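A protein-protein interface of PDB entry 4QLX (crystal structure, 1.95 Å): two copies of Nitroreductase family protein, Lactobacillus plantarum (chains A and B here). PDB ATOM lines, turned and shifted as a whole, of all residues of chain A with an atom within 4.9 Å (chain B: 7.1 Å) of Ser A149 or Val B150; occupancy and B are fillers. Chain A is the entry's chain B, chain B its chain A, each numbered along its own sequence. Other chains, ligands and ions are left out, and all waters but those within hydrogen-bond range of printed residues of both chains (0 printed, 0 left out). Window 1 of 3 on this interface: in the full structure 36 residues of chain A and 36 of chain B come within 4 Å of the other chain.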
ATOM      1  N   THR A 145       0.042  26.039  15.651  1.00  0.00           N
ATOM      2  CA  THR A 145      -0.234  24.696  16.167  1.00  0.00           C
ATOM      3  C   THR A 145       0.808  23.697  15.644  1.00  0.00           C
ATOM      4  O   THR A 145       1.324  22.864  16.399  1.00  0.00           O
ATOM      5  CB  THR A 145      -1.650  24.226  15.778  1.00  0.00           C
ATOM      6  OG1 THR A 145      -2.621  25.089  16.385  1.00  0.00           O
ATOM      7  CG2 THR A 145      -1.897  22.796  16.238  1.00  0.00           C
ATOM      8  N   ILE A 146       1.130  23.796  14.359  1.00  0.00           N
ATOM      9  CA  ILE A 146       2.115  22.901  13.770  1.00  0.00           C
ATOM     10  C   ILE A 146       3.480  23.047  14.437  1.00  0.00           C
ATOM     11  O   ILE A 146       4.054  22.053  14.871  1.00  0.00           O
ATOM     12  CB  ILE A 146       2.261  23.130  12.263  1.00  0.00           C
ATOM     13  CG1 ILE A 146       0.981  22.688  11.544  1.00  0.00           C
ATOM     14  CG2 ILE A 146       3.441  22.349  11.749  1.00  0.00           C
ATOM     15  CD1 ILE A 146       1.028  22.857  10.033  1.00  0.00           C
ATOM     16  N   ASP A 147       3.986  24.280  14.528  1.00  0.00           N
ATOM     17  CA  ASP A 147       5.228  24.557  15.276  1.00  0.00           C
ATOM     18  C   ASP A 147       5.182  23.988  16.690  1.00  0.00           C
ATOM     19  O   ASP A 147       6.133  23.351  17.156  1.00  0.00           O
ATOM     20  CB  ASP A 147       5.500  26.066  15.378  1.00  0.00           C
ATOM     21  CG  ASP A 147       5.860  26.712  14.044  1.00  0.00           C
ATOM     22  OD1 ASP A 147       5.836  26.022  12.991  1.00  0.00           O
ATOM     23  OD2 ASP A 147       6.166  27.937  14.068  1.00  0.00           O
ATOM     24  N   CYS A 148       4.078  24.247  17.385  1.00  0.00           N
ATOM     25  CA  CYS A 148       3.924  23.808  18.769  1.00  0.00           C
ATOM     26  C   CYS A 148       3.955  22.294  18.901  1.00  0.00           C
ATOM     27  O   CYS A 148       4.459  21.749  19.893  1.00  0.00           O
ATOM     28  CB  CYS A 148       2.624  24.345  19.358  1.00  0.00           C
ATOM     29  SG  CYS A 148       2.762  26.084  19.798  1.00  0.00           S
ATOM     30  N   SER A 149       3.421  21.617  17.894  1.00  0.00           N
ATOM     31  CA  SER A 149       3.374  20.161  17.931  1.00  0.00           C
ATOM     32  C   SER A 149       4.739  19.553  17.651  1.00  0.00           C
ATOM     33  O   SER A 149       5.087  18.526  18.228  1.00  0.00           O
ATOM     34  CB  SER A 149       2.336  19.642  16.936  1.00  0.00           C
ATOM     35  OG  SER A 149       1.063  20.222  17.180  1.00  0.00           O
ATOM     36  N   VAL A 150       5.545  20.171  16.785  1.00  0.00           N
ATOM     37  CA  VAL A 150       6.814  19.532  16.504  1.00  0.00           C
ATOM     38  C   VAL A 150       7.768  19.749  17.683  1.00  0.00           C
ATOM     39  O   VAL A 150       8.544  18.849  18.028  1.00  0.00           O
ATOM     40  CB  VAL A 150       7.443  20.016  15.171  1.00  0.00           C
ATOM     41  CG1 VAL A 150       6.537  19.605  13.998  1.00  0.00           C
ATOM     42  CG2 VAL A 150       7.703  21.522  15.168  1.00  0.00           C
ATOM     43  N   VAL A 151       7.704  20.912  18.330  1.00  0.00           N
ATOM     44  CA  VAL A 151       8.588  21.114  19.476  1.00  0.00           C
ATOM     45  C   VAL A 151       8.061  20.230  20.623  1.00  0.00           C
ATOM     46  O   VAL A 151       8.835  19.704  21.423  1.00  0.00           O
ATOM     47  CB  VAL A 151       8.726  22.638  19.875  1.00  0.00           C
ATOM     48  CG1 VAL A 151       7.477  23.182  20.559  1.00  0.00           C
ATOM     49  CG2 VAL A 151       9.963  22.851  20.751  1.00  0.00           C
ATOM     50  N   GLY A 152       6.750  20.003  20.660  1.00  0.00           N
ATOM     51  CA  GLY A 152       6.168  19.110  21.653  1.00  0.00           C
ATOM     52  C   GLY A 152       6.672  17.688  21.497  1.00  0.00           C
ATOM     53  O   GLY A 152       7.019  17.028  22.479  1.00  0.00           O
ATOM     54  N   MET A 153       6.738  17.220  20.248  1.00  0.00           N
ATOM     55  CA  MET A 153       7.273  15.891  19.958  1.00  0.00           C
ATOM     56  C   MET A 153       8.744  15.783  20.380  1.00  0.00           C
ATOM     57  O   MET A 153       9.175  14.785  20.969  1.00  0.00           O
ATOM     58  CB  MET A 153       7.123  15.564  18.461  1.00  0.00           C
ATOM     59  CG  MET A 153       7.554  14.131  18.075  1.00  0.00           C
ATOM     60  SD  MET A 153       6.503  12.857  18.831  1.00  0.00           S
ATOM     61  CE  MET A 153       7.621  12.185  20.076  1.00  0.00           C
ATOM     62  N   VAL A 191      -2.325  24.507  22.773  1.00  0.00           N
ATOM     63  CA  VAL A 191      -2.108  23.353  21.914  1.00  0.00           C
ATOM     64  C   VAL A 191      -2.065  22.048  22.703  1.00  0.00           C
ATOM     65  O   VAL A 191      -2.883  21.170  22.479  1.00  0.00           O
ATOM     66  CB  VAL A 191      -0.813  23.501  21.096  1.00  0.00           C
ATOM     67  CG1 VAL A 191      -0.610  22.281  20.171  1.00  0.00           C
ATOM     68  CG2 VAL A 191      -0.856  24.784  20.301  1.00  0.00           C
ATOM     69  N   MET A 192      -1.122  21.927  23.629  1.00  0.00           N
ATOM     70  CA  MET A 192      -0.966  20.678  24.379  1.00  0.00           C
ATOM     71  C   MET A 192      -0.118  20.866  25.618  1.00  0.00           C
ATOM     72  O   MET A 192       0.687  21.776  25.678  1.00  0.00           O
ATOM     73  CB  MET A 192      -0.319  19.602  23.510  1.00  0.00           C
ATOM     74  CG  MET A 192       1.193  19.809  23.252  1.00  0.00           C
ATOM     75  SD  MET A 192       1.942  18.435  22.329  1.00  0.00           S
ATOM     76  CE  MET A 192       1.045  18.597  20.800  1.00  0.00           C
ATOM     77  N   ALA B  46       8.485   6.276  12.036  1.00  0.00           N
ATOM     78  CA  ALA B  46       7.910   7.554  12.454  1.00  0.00           C
ATOM     79  C   ALA B  46       6.549   7.392  13.140  1.00  0.00           C
ATOM     80  O   ALA B  46       6.189   8.172  14.023  1.00  0.00           O
ATOM     81  CB  ALA B  46       7.775   8.485  11.259  1.00  0.00           C
ATOM     82  N   ALA B  49       5.116   7.414  16.713  1.00  0.00           N
ATOM     83  CA  ALA B  49       4.683   8.668  17.350  1.00  0.00           C
ATOM     84  C   ALA B  49       3.364   8.534  18.142  1.00  0.00           C
ATOM     85  O   ALA B  49       2.531   7.681  17.825  1.00  0.00           O
ATOM     86  CB  ALA B  49       4.543   9.780  16.268  1.00  0.00           C
ATOM     87  N   PRO B  50       3.169   9.385  19.174  1.00  0.00           N
ATOM     88  CA  PRO B  50       1.886   9.430  19.888  1.00  0.00           C
ATOM     89  C   PRO B  50       0.837  10.117  19.027  1.00  0.00           C
ATOM     90  O   PRO B  50       1.181  10.755  18.038  1.00  0.00           O
ATOM     91  CB  PRO B  50       2.202  10.277  21.122  1.00  0.00           C
ATOM     92  CG  PRO B  50       3.213  11.248  20.594  1.00  0.00           C
ATOM     93  CD  PRO B  50       4.099  10.408  19.684  1.00  0.00           C
ATOM     94  N   SER B  51      -0.427   9.986  19.403  1.00  0.00           N
ATOM     95  CA  SER B  51      -1.530  10.594  18.673  1.00  0.00           C
ATOM     96  C   SER B  51      -2.684  10.688  19.659  1.00  0.00           C
ATOM     97  O   SER B  51      -2.776   9.864  20.582  1.00  0.00           O
ATOM     98  CB  SER B  51      -1.911   9.769  17.429  1.00  0.00           C
ATOM     99  OG  SER B  51      -2.417   8.494  17.808  1.00  0.00           O
ATOM    100  N   ALA B  52      -3.542  11.690  19.499  1.00  0.00           N
ATOM    101  CA  ALA B  52      -4.659  11.841  20.433  1.00  0.00           C
ATOM    102  C   ALA B  52      -5.538  10.600  20.396  1.00  0.00           C
ATOM    103  O   ALA B  52      -5.946  10.152  19.326  1.00  0.00           O
ATOM    104  CB  ALA B  52      -5.480  13.097  20.114  1.00  0.00           C
ATOM    105  N   TRP B  58      -3.205  10.278  10.821  1.00  0.00           N
ATOM    106  CA  TRP B  58      -2.318  10.723   9.741  1.00  0.00           C
ATOM    107  C   TRP B  58      -2.487   9.856   8.507  1.00  0.00           C
ATOM    108  O   TRP B  58      -2.912   8.709   8.603  1.00  0.00           O
ATOM    109  CB  TRP B  58      -0.854  10.694  10.187  1.00  0.00           C
ATOM    110  CG  TRP B  58      -0.470   9.490  11.024  1.00  0.00           C
ATOM    111  CD1 TRP B  58      -0.427   8.184  10.616  1.00  0.00           C
ATOM    112  CD2 TRP B  58      -0.050   9.493  12.392  1.00  0.00           C
ATOM    113  NE1 TRP B  58      -0.008   7.381  11.642  1.00  0.00           N
ATOM    114  CE2 TRP B  58       0.236   8.160  12.748  1.00  0.00           C
ATOM    115  CE3 TRP B  58       0.125  10.497  13.355  1.00  0.00           C
ATOM    116  CZ2 TRP B  58       0.668   7.792  14.026  1.00  0.00           C
ATOM    117  CZ3 TRP B  58       0.559  10.137  14.629  1.00  0.00           C
ATOM    118  CH2 TRP B  58       0.829   8.791  14.949  1.00  0.00           C
ATOM    119  N   PHE B 142      -7.906  20.560  13.552  1.00  0.00           N
ATOM    120  CA  PHE B 142      -6.910  20.912  14.560  1.00  0.00           C
ATOM    121  C   PHE B 142      -6.306  19.663  15.201  1.00  0.00           C
ATOM    122  O   PHE B 142      -5.078  19.523  15.298  1.00  0.00           O
ATOM    123  CB  PHE B 142      -7.570  21.817  15.613  1.00  0.00           C
ATOM    124  CG  PHE B 142      -6.755  22.024  16.862  1.00  0.00           C
ATOM    125  CD1 PHE B 142      -5.741  22.973  16.893  1.00  0.00           C
ATOM    126  CD2 PHE B 142      -7.029  21.302  18.015  1.00  0.00           C
ATOM    127  CE1 PHE B 142      -4.996  23.178  18.047  1.00  0.00           C
ATOM    128  CE2 PHE B 142      -6.288  21.501  19.171  1.00  0.00           C
ATOM    129  CZ  PHE B 142      -5.270  22.446  19.184  1.00  0.00           C
ATOM    130  N   ALA B 144      -6.375  16.561  13.985  1.00  0.00           N
ATOM    131  CA  ALA B 144      -5.640  15.773  13.014  1.00  0.00           C
ATOM    132  C   ALA B 144      -4.312  16.468  12.684  1.00  0.00           C
ATOM    133  O   ALA B 144      -3.301  15.802  12.469  1.00  0.00           O
ATOM    134  CB  ALA B 144      -6.478  15.553  11.757  1.00  0.00           C
ATOM    135  N   THR B 145      -4.308  17.800  12.672  1.00  0.00           N
ATOM    136  CA  THR B 145      -3.078  18.553  12.354  1.00  0.00           C
ATOM    137  C   THR B 145      -1.982  18.293  13.395  1.00  0.00           C
ATOM    138  O   THR B 145      -0.808  18.108  13.051  1.00  0.00           O
ATOM    139  CB  THR B 145      -3.352  20.084  12.237  1.00  0.00           C
ATOM    140  OG1 THR B 145      -4.206  20.347  11.111  1.00  0.00           O
ATOM    141  CG2 THR B 145      -2.056  20.871  12.077  1.00  0.00           C
ATOM    142  N   ILE B 146      -2.357  18.241  14.665  1.00  0.00           N
ATOM    143  CA  ILE B 146      -1.378  17.926  15.700  1.00  0.00           C
ATOM    144  C   ILE B 146      -0.746  16.540  15.509  1.00  0.00           C
ATOM    145  O   ILE B 146       0.469  16.422  15.543  1.00  0.00           O
ATOM    146  CB  ILE B 146      -1.996  17.997  17.105  1.00  0.00           C
ATOM    147  CG1 ILE B 146      -2.505  19.407  17.394  1.00  0.00           C
ATOM    148  CG2 ILE B 146      -0.962  17.597  18.149  1.00  0.00           C
ATOM    149  CD1 ILE B 146      -3.232  19.532  18.743  1.00  0.00           C
ATOM    150  N   ASP B 147      -1.566  15.504  15.307  1.00  0.00           N
ATOM    151  CA  ASP B 147      -1.048  14.152  15.038  1.00  0.00           C
ATOM    152  C   ASP B 147      -0.067  14.141  13.838  1.00  0.00           C
ATOM    153  O   ASP B 147       0.980  13.495  13.868  1.00  0.00           O
ATOM    154  CB  ASP B 147      -2.183  13.172  14.743  1.00  0.00           C
ATOM    155  CG  ASP B 147      -3.067  12.866  15.957  1.00  0.00           C
ATOM    156  OD1 ASP B 147      -2.795  13.346  17.084  1.00  0.00           O
ATOM    157  OD2 ASP B 147      -4.058  12.127  15.758  1.00  0.00           O
ATOM    158  N   CYS B 148      -0.431  14.848  12.779  1.00  0.00           N
ATOM    159  CA  CYS B 148       0.382  14.863  11.563  1.00  0.00           C
ATOM    160  C   CYS B 148       1.710  15.566  11.778  1.00  0.00           C
ATOM    161  O   CYS B 148       2.704  15.263  11.122  1.00  0.00           O
ATOM    162  CB  CYS B 148      -0.370  15.544  10.430  1.00  0.00           C
ATOM    163  SG  CYS B 148      -1.689  14.538   9.756  1.00  0.00           S
ATOM    164  N   SER B 149       1.710  16.526  12.690  1.00  0.00           N
ATOM    165  CA  SER B 149       2.918  17.292  12.973  1.00  0.00           C
ATOM    166  C   SER B 149       3.876  16.479  13.835  1.00  0.00           C
ATOM    167  O   SER B 149       5.084  16.539  13.638  1.00  0.00           O
ATOM    168  CB  SER B 149       2.558  18.623  13.657  1.00  0.00           C
ATOM    169  OG  SER B 149       1.636  19.364  12.867  1.00  0.00           O
ATOM    170  N   VAL B 150       3.360  15.709  14.796  1.00  0.00           N
ATOM    171  CA  VAL B 150       4.292  14.948  15.625  1.00  0.00           C
ATOM    172  C   VAL B 150       4.864  13.764  14.855  1.00  0.00           C
ATOM    173  O   VAL B 150       6.021  13.390  15.083  1.00  0.00           O
ATOM    174  CB  VAL B 150       3.669  14.447  16.962  1.00  0.00           C
ATOM    175  CG1 VAL B 150       3.182  15.631  17.807  1.00  0.00           C
ATOM    176  CG2 VAL B 150       2.540  13.424  16.727  1.00  0.00           C
ATOM    177  N   VAL B 151       4.086  13.165  13.950  1.00  0.00           N
ATOM    178  CA  VAL B 151       4.640  12.072  13.158  1.00  0.00           C
ATOM    179  C   VAL B 151       5.611  12.655  12.117  1.00  0.00           C
ATOM    180  O   VAL B 151       6.625  12.034  11.787  1.00  0.00           O
ATOM    181  CB  VAL B 151       3.529  11.190  12.483  1.00  0.00           C
ATOM    182  CG1 VAL B 151       2.934  11.869  11.257  1.00  0.00           C
ATOM    183  CG2 VAL B 151       4.097   9.834  12.078  1.00  0.00           C
ATOM    184  N   GLY B 152       5.329  13.862  11.630  1.00  0.00           N
ATOM    185  CA  GLY B 152       6.236  14.527  10.695  1.00  0.00           C
ATOM    186  C   GLY B 152       7.583  14.838  11.322  1.00  0.00           C
ATOM    187  O   GLY B 152       8.650  14.643  10.720  1.00  0.00           O
ATOM    188  N   MET B 153       7.530  15.342  12.548  1.00  0.00           N
ATOM    189  CA  MET B 153       8.742  15.592  13.322  1.00  0.00           C
ATOM    190  C   MET B 153       9.534  14.300  13.519  1.00  0.00           C
ATOM    191  O   MET B 153      10.744  14.294  13.390  1.00  0.00           O
ATOM    192  CB  MET B 153       8.396  16.217  14.685  1.00  0.00           C
ATOM    193  CG  MET B 153       9.641  16.684  15.499  1.00  0.00           C
ATOM    194  SD  MET B 153      10.596  18.005  14.707  1.00  0.00           S
ATOM    195  CE  MET B 153      12.115  17.150  14.275  1.00  0.00           C
ATOM    196  N   GLN B 154       8.862  13.189  13.818  1.00  0.00           N
ATOM    197  CA  GLN B 154       9.615  11.952  13.994  1.00  0.00           C
ATOM    198  C   GLN B 154      10.216  11.510  12.660  1.00  0.00           C
ATOM    199  O   GLN B 154      11.325  10.993  12.635  1.00  0.00           O
ATOM    200  CB  GLN B 154       8.748  10.842  14.617  1.00  0.00           C
ATOM    201  CG  GLN B 154       8.522  11.088  16.115  1.00  0.00           C
ATOM    202  CD  GLN B 154       8.515   9.815  16.958  1.00  0.00           C
ATOM    203  OE1 GLN B 154       9.022   9.806  18.084  1.00  0.00           O
ATOM    204  NE2 GLN B 154       7.945   8.732  16.416  1.00  0.00           N
ATOM    205  N   LEU B 155       9.512  11.762  11.557  1.00  0.00           N
ATOM    206  CA  LEU B 155       9.994  11.312  10.251  1.00  0.00           C
ATOM    207  C   LEU B 155      11.268  12.089   9.856  1.00  0.00           C
ATOM    208  O   LEU B 155      12.178  11.539   9.224  1.00  0.00           O
ATOM    209  CB  LEU B 155       8.895  11.467   9.186  1.00  0.00           C
ATOM    210  CG  LEU B 155       9.206  10.940   7.772  1.00  0.00           C
ATOM    211  CD1 LEU B 155       9.756   9.517   7.821  1.00  0.00           C
ATOM    212  CD2 LEU B 155       7.974  10.990   6.889  1.00  0.00           C
ATOM    213  N   MET B 192       1.589  18.984   5.773  1.00  0.00           N
ATOM    214  CA  MET B 192       2.958  19.295   5.367  1.00  0.00           C
ATOM    215  C   MET B 192       3.572  18.209   4.492  1.00  0.00           C
ATOM    216  O   MET B 192       3.193  17.043   4.568  1.00  0.00           O
ATOM    217  CB  MET B 192       3.858  19.529   6.596  1.00  0.00           C
ATOM    218  CG  MET B 192       4.107  18.270   7.442  1.00  0.00           C
ATOM    219  SD  MET B 192       5.325  18.447   8.774  1.00  0.00           S
ATOM    220  CE  MET B 192       4.345  19.278  10.027  1.00  0.00           C
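The backbone carbonyl oxygen of Thr A145 lies within hydrogen-bond range of the side-chain hydroxyl of Ser A149 (2.8 Å).
The side-chain hydroxyl (OG) of Ser B149 is in hydrogen-bond range of the backbone carbonyl oxygen (O) of Thr B145.
The backbone carbonyl oxygen of Ala B46 lies within hydrogen-bond range of the side-chain amide nitrogen of Gln B154 (3.0 Å).
N of Ala B49 sits close to NE2 of Gln B154, at 3.1 Å.
Among the printed residues, pairs that only touch across the chains: Thr A145 with Phe B142 (3.5 Å), Thr A145 with Ile B146 (3.6 Å), Ile A146 with Thr B145 (3.6 Å), Ile A146 with Ser B149 (3.6 Å), Ile A146 with Met B192 (3.6 Å), Ser A149 with Ile B146 (3.5 Å), Ser A149 with Ser B149 (3.4 Å), Ser A149 with Val B150 (3.5 Å), Val A150 with Ser B149 (3.4 Å), Val A150 with Met B153 (3.5 Å), Met A153 with Pro B50 (3.5 Å), Met A153 with Val B150 (3.4 Å), Met A153 with Gln B154 (3.4 Å) and Met A192 with Ile B146 (3.5 Å).
Ser A149 touches three residues of chain B.
Printed residues of chain A within 4 Å of Val B150: Ser A149 (3.5 Å) and Met A153 (3.4 Å).
Printed residues of chain A within 4 Å of Pro B50: Met A153.
Of the printed residues of chain A, Met B192 touches Ile A146.
Of the printed residues of chain A, Phe B142 touches Thr A145 (3.5 Å).
Of the printed residues of chain A, Thr B145 touches Ile A146.
Printed residues of chain A within 4 Å of Gln B154: Met A153 (3.4 Å).
Val A191 touches none of the printed residues of chain B.
The nearest residue of chain B that does not touch Ser A149 is Thr B145 (5.0 Å).
The nearest printed residue of chain B that does not touch Met A153 is Met B153 (4.04 Å).
Of the 11 printed residues of chain A, 6 touch a printed residue of chain B.
Hydrophobic or aromatic side chains of chain A that line the printed part of chain B: Ile A146, Val A150, Met A153 and Met A192.
Of the 20 printed residues of chain B, 9 touch a printed residue of chain A.
Printed residues of chain B that touch a printed residue of chain A: Pro B50, Phe B142, Thr B145, Ile B146, Ser B149, Val B150, Met B153, Gln B154 and Met B192.
Hydrophobic or aromatic side chains of chain B within 4 Å of the printed part of chain A: Pro B50, Phe B142, Ile B146, Val B150, Met B153 and Met B192.
Ile A146 touches Ser B149, and with the chains exchanged Ser A149 touches Ile B146.
Ile A146 touches Met B192, and with the chains exchanged Met A192 touches Ile B146.
Ser A149 touches its own counterpart, Ser B149.
Ser A149 touches Val B150, and with the chains exchanged Val A150 touches Ser B149.
Of the 14 pairs that touch across the chains among the printed residues, 11 have their exchanged pair printed and touching as well.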
